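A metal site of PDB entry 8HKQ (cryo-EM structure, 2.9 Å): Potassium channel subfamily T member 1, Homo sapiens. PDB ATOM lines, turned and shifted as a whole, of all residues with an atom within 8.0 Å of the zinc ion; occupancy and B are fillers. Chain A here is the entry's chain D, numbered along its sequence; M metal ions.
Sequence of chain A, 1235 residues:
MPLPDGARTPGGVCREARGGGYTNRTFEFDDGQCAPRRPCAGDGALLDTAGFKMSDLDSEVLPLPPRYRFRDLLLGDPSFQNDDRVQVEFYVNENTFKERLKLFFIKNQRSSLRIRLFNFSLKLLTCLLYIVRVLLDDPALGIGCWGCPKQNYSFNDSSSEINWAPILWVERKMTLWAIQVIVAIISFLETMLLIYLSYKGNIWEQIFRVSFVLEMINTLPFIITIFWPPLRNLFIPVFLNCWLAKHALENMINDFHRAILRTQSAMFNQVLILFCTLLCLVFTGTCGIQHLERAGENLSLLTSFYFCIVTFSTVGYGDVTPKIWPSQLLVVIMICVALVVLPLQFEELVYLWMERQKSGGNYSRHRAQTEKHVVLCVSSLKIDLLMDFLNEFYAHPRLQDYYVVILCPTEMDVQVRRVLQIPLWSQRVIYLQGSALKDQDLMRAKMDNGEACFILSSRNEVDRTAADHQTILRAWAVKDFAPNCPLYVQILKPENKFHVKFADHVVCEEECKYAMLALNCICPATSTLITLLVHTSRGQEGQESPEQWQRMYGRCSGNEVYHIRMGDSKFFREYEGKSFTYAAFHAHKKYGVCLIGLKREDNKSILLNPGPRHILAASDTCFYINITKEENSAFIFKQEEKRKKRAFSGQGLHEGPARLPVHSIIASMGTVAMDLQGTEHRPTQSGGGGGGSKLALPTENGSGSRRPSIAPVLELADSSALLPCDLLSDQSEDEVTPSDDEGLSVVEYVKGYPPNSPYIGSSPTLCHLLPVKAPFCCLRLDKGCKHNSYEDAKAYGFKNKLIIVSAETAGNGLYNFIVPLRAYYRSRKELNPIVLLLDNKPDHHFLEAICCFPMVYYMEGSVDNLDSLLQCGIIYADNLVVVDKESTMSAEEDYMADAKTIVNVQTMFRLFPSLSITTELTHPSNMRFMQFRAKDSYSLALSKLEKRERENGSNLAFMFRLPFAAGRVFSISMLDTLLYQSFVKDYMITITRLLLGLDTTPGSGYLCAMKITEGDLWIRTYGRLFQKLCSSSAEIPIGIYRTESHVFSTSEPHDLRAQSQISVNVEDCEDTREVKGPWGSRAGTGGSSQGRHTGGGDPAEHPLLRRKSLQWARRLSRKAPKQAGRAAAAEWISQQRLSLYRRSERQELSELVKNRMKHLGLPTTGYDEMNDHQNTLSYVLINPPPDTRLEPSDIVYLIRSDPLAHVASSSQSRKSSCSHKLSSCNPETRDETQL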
ATOM      1  N   ALA A 774      -7.964  16.369 -19.945  1.00  0.00           N
ATOM      2  CA  ALA A 774      -8.565  17.386 -19.088  1.00  0.00           C
ATOM      3  C   ALA A 774     -10.083  17.404 -19.277  1.00  0.00           C
ATOM      4  O   ALA A 774     -10.561  17.307 -20.415  1.00  0.00           O
ATOM      5  CB  ALA A 774      -7.998  18.769 -19.404  1.00  0.00           C
ATOM      6  N   PRO A 775     -10.843  17.513 -18.198  1.00  0.00           N
ATOM      7  CA  PRO A 775     -12.292  17.636 -18.321  1.00  0.00           C
ATOM      8  C   PRO A 775     -12.665  18.931 -19.033  1.00  0.00           C
ATOM      9  O   PRO A 775     -11.929  19.925 -19.023  1.00  0.00           O
ATOM     10  CB  PRO A 775     -12.790  17.639 -16.872  1.00  0.00           C
ATOM     11  CG  PRO A 775     -11.579  17.956 -16.043  1.00  0.00           C
ATOM     12  CD  PRO A 775     -10.408  17.418 -16.791  1.00  0.00           C
ATOM     13  N   PHE A 776     -13.840  18.914 -19.669  1.00  0.00           N
ATOM     14  CA  PHE A 776     -14.304  20.055 -20.445  1.00  0.00           C
ATOM     15  C   PHE A 776     -14.508  21.306 -19.595  1.00  0.00           C
ATOM     16  O   PHE A 776     -14.543  22.410 -20.148  1.00  0.00           O
ATOM     17  CB  PHE A 776     -15.609  19.709 -21.168  1.00  0.00           C
ATOM     18  CG  PHE A 776     -15.429  18.850 -22.387  1.00  0.00           C
ATOM     19  CD1 PHE A 776     -14.273  18.116 -22.575  1.00  0.00           C
ATOM     20  CD2 PHE A 776     -16.433  18.761 -23.334  1.00  0.00           C
ATOM     21  CE1 PHE A 776     -14.111  17.318 -23.690  1.00  0.00           C
ATOM     22  CE2 PHE A 776     -16.279  17.971 -24.458  1.00  0.00           C
ATOM     23  CZ  PHE A 776     -15.117  17.242 -24.633  1.00  0.00           C
ATOM     24  N   CYS A 777     -14.638  21.153 -18.269  1.00  0.00           N
ATOM     25  CA  CYS A 777     -14.782  22.312 -17.401  1.00  0.00           C
ATOM     26  C   CYS A 777     -13.454  23.012 -17.161  1.00  0.00           C
ATOM     27  O   CYS A 777     -13.419  24.241 -17.002  1.00  0.00           O
ATOM     28  CB  CYS A 777     -15.386  21.885 -16.060  1.00  0.00           C
ATOM     29  SG  CYS A 777     -14.267  20.920 -15.022  1.00  0.00           S
ATOM     30  N   CYS A 778     -12.346  22.261 -17.137  1.00  0.00           N
ATOM     31  CA  CYS A 778     -11.041  22.832 -16.838  1.00  0.00           C
ATOM     32  C   CYS A 778     -10.425  23.565 -18.020  1.00  0.00           C
ATOM     33  O   CYS A 778      -9.369  24.187 -17.863  1.00  0.00           O
ATOM     34  CB  CYS A 778     -10.095  21.726 -16.361  1.00  0.00           C
ATOM     35  SG  CYS A 778     -10.414  21.161 -14.678  1.00  0.00           S
ATOM     36  N   LEU A 779     -11.044  23.500 -19.197  1.00  0.00           N
ATOM     37  CA  LEU A 779     -10.549  24.201 -20.373  1.00  0.00           C
ATOM     38  C   LEU A 779     -11.077  25.617 -20.489  1.00  0.00           C
ATOM     39  O   LEU A 779     -10.809  26.281 -21.494  1.00  0.00           O
ATOM     40  CB  LEU A 779     -10.913  23.413 -21.638  1.00  0.00           C
ATOM     41  CG  LEU A 779     -10.334  22.006 -21.779  1.00  0.00           C
ATOM     42  CD1 LEU A 779     -11.055  21.244 -22.889  1.00  0.00           C
ATOM     43  CD2 LEU A 779      -8.846  22.054 -22.051  1.00  0.00           C
ATOM     44  N   ARG A 780     -11.800  26.105 -19.488  1.00  0.00           N
ATOM     45  CA  ARG A 780     -12.512  27.374 -19.560  1.00  0.00           C
ATOM     46  C   ARG A 780     -11.869  28.363 -18.595  1.00  0.00           C
ATOM     47  O   ARG A 780     -11.758  28.086 -17.398  1.00  0.00           O
ATOM     48  CB  ARG A 780     -13.992  27.188 -19.228  1.00  0.00           C
ATOM     49  CG  ARG A 780     -14.876  28.360 -19.569  1.00  0.00           C
ATOM     50  CD  ARG A 780     -16.307  27.911 -19.779  1.00  0.00           C
ATOM     51  NE  ARG A 780     -17.274  28.911 -19.347  1.00  0.00           N
ATOM     52  CZ  ARG A 780     -17.680  29.936 -20.081  1.00  0.00           C
ATOM     53  NH1 ARG A 780     -17.217  30.127 -21.309  1.00  0.00           N
ATOM     54  NH2 ARG A 780     -18.572  30.787 -19.585  1.00  0.00           N
ATOM     55  N   LYS A 783     -15.352  30.475 -16.265  1.00  0.00           N
ATOM     56  CA  LYS A 783     -16.014  29.938 -15.085  1.00  0.00           C
ATOM     57  C   LYS A 783     -15.056  29.121 -14.231  1.00  0.00           C
ATOM     58  O   LYS A 783     -14.059  28.575 -14.726  1.00  0.00           O
ATOM     59  CB  LYS A 783     -17.215  29.078 -15.481  1.00  0.00           C
ATOM     60  CG  LYS A 783     -18.295  29.829 -16.247  1.00  0.00           C
ATOM     61  CD  LYS A 783     -19.590  29.027 -16.432  1.00  0.00           C
ATOM     62  CE  LYS A 783     -20.260  28.598 -15.121  1.00  0.00           C
ATOM     63  NZ  LYS A 783     -19.572  27.516 -14.349  1.00  0.00           N
ATOM     64  N   GLY A 784     -15.371  29.044 -12.945  1.00  0.00           N
ATOM     65  CA  GLY A 784     -14.664  28.160 -12.050  1.00  0.00           C
ATOM     66  C   GLY A 784     -15.320  26.798 -11.993  1.00  0.00           C
ATOM     67  O   GLY A 784     -16.483  26.631 -12.339  1.00  0.00           O
ATOM     68  N   CYS A 785     -14.547  25.804 -11.564  1.00  0.00           N
ATOM     69  CA  CYS A 785     -15.044  24.427 -11.535  1.00  0.00           C
ATOM     70  C   CYS A 785     -14.682  23.738 -10.223  1.00  0.00           C
ATOM     71  O   CYS A 785     -14.206  24.389  -9.289  1.00  0.00           O
ATOM     72  CB  CYS A 785     -14.481  23.637 -12.723  1.00  0.00           C
ATOM     73  SG  CYS A 785     -12.682  23.669 -12.854  1.00  0.00           S
ATOM     74  N   LYS A 786     -14.913  22.437 -10.156  1.00  0.00           N
ATOM     75  CA  LYS A 786     -14.560  21.683  -8.952  1.00  0.00           C
ATOM     76  C   LYS A 786     -13.062  21.698  -8.712  1.00  0.00           C
ATOM     77  O   LYS A 786     -12.614  21.837  -7.563  1.00  0.00           O
ATOM     78  CB  LYS A 786     -15.066  20.247  -9.073  1.00  0.00           C
ATOM     79  CG  LYS A 786     -16.554  20.134  -9.377  1.00  0.00           C
ATOM     80  CD  LYS A 786     -17.394  20.659  -8.230  1.00  0.00           C
ATOM     81  CE  LYS A 786     -18.429  19.641  -7.796  1.00  0.00           C
ATOM     82  NZ  LYS A 786     -19.372  20.199  -6.789  1.00  0.00           N
ATOM     83  N   HIS A 787     -12.273  21.559  -9.776  1.00  0.00           N
ATOM     84  CA  HIS A 787     -10.825  21.503  -9.652  1.00  0.00           C
ATOM     85  C   HIS A 787     -10.166  22.874  -9.524  1.00  0.00           C
ATOM     86  O   HIS A 787      -9.100  22.984  -8.912  1.00  0.00           O
ATOM     87  CB  HIS A 787     -10.223  20.771 -10.858  1.00  0.00           C
ATOM     88  CG  HIS A 787     -11.113  19.716 -11.430  1.00  0.00           C
ATOM     89  ND1 HIS A 787     -12.146  20.009 -12.293  1.00  0.00           N
ATOM     90  CD2 HIS A 787     -11.126  18.379 -11.261  1.00  0.00           C
ATOM     91  CE1 HIS A 787     -12.764  18.885 -12.629  1.00  0.00           C
ATOM     92  NE2 HIS A 787     -12.159  17.885 -12.021  1.00  0.00           N
ATOM     93  N   ASN A 788     -10.785  23.918 -10.087  1.00  0.00           N
ATOM     94  CA  ASN A 788     -10.210  25.253 -10.035  1.00  0.00           C
ATOM     95  C   ASN A 788     -11.334  26.279  -9.966  1.00  0.00           C
ATOM     96  O   ASN A 788     -12.363  26.125 -10.630  1.00  0.00           O
ATOM     97  CB  ASN A 788      -9.325  25.537 -11.261  1.00  0.00           C
ATOM     98  CG  ASN A 788      -8.035  24.732 -11.243  1.00  0.00           C
ATOM     99  OD1 ASN A 788      -7.267  24.782 -10.286  1.00  0.00           O
ATOM    100  ND2 ASN A 788      -7.801  23.979 -12.313  1.00  0.00           N
ATOM    101  N   SER A 789     -11.125  27.323  -9.166  1.00  0.00           N
ATOM    102  CA  SER A 789     -12.086  28.415  -9.043  1.00  0.00           C
ATOM    103  C   SER A 789     -11.612  29.690  -9.738  1.00  0.00           C
ATOM    104  O   SER A 789     -12.247  30.738  -9.589  1.00  0.00           O
ATOM    105  CB  SER A 789     -12.367  28.706  -7.564  1.00  0.00           C
ATOM    106  OG  SER A 789     -13.278  29.778  -7.420  1.00  0.00           O
ATOM    107  N   TYR A 796      -4.673  32.171 -12.533  1.00  0.00           N
ATOM    108  CA  TYR A 796      -3.921  30.980 -12.919  1.00  0.00           C
ATOM    109  C   TYR A 796      -2.436  31.123 -12.615  1.00  0.00           C
ATOM    110  O   TYR A 796      -1.776  30.124 -12.286  1.00  0.00           O
ATOM    111  CB  TYR A 796      -4.138  30.681 -14.401  1.00  0.00           C
ATOM    112  CG  TYR A 796      -5.375  29.857 -14.694  1.00  0.00           C
ATOM    113  CD1 TYR A 796      -6.615  30.450 -14.799  1.00  0.00           C
ATOM    114  CD2 TYR A 796      -5.280  28.482 -14.865  1.00  0.00           C
ATOM    115  CE1 TYR A 796      -7.750  29.697 -15.064  1.00  0.00           C
ATOM    116  CE2 TYR A 796      -6.408  27.723 -15.132  1.00  0.00           C
ATOM    117  CZ  TYR A 796      -7.636  28.331 -15.230  1.00  0.00           C
ATOM    118  OH  TYR A 796      -8.758  27.579 -15.493  1.00  0.00           O
HETATM  119 ZN    ZN M   1     -12.473  21.511 -13.673  1.00  0.00          ZN
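The zinc ion is bound by a ring nitrogen (ND1) of His 787, the side-chain sulfur (SG) of Cys 785, the side-chain sulfur (SG) of Cys 778 and the side-chain sulfur (SG) of Cys 777.
Of the 15 residues printed, 4 come within 4 Å of the zinc ion. The nearest printed residue that does not touch the zinc ion is Pro 775 (4.4 Å).
The side-chain sulfur of Cys 785 sits close to the backbone carbonyl oxygen of Asn 788 (3.3 Å).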
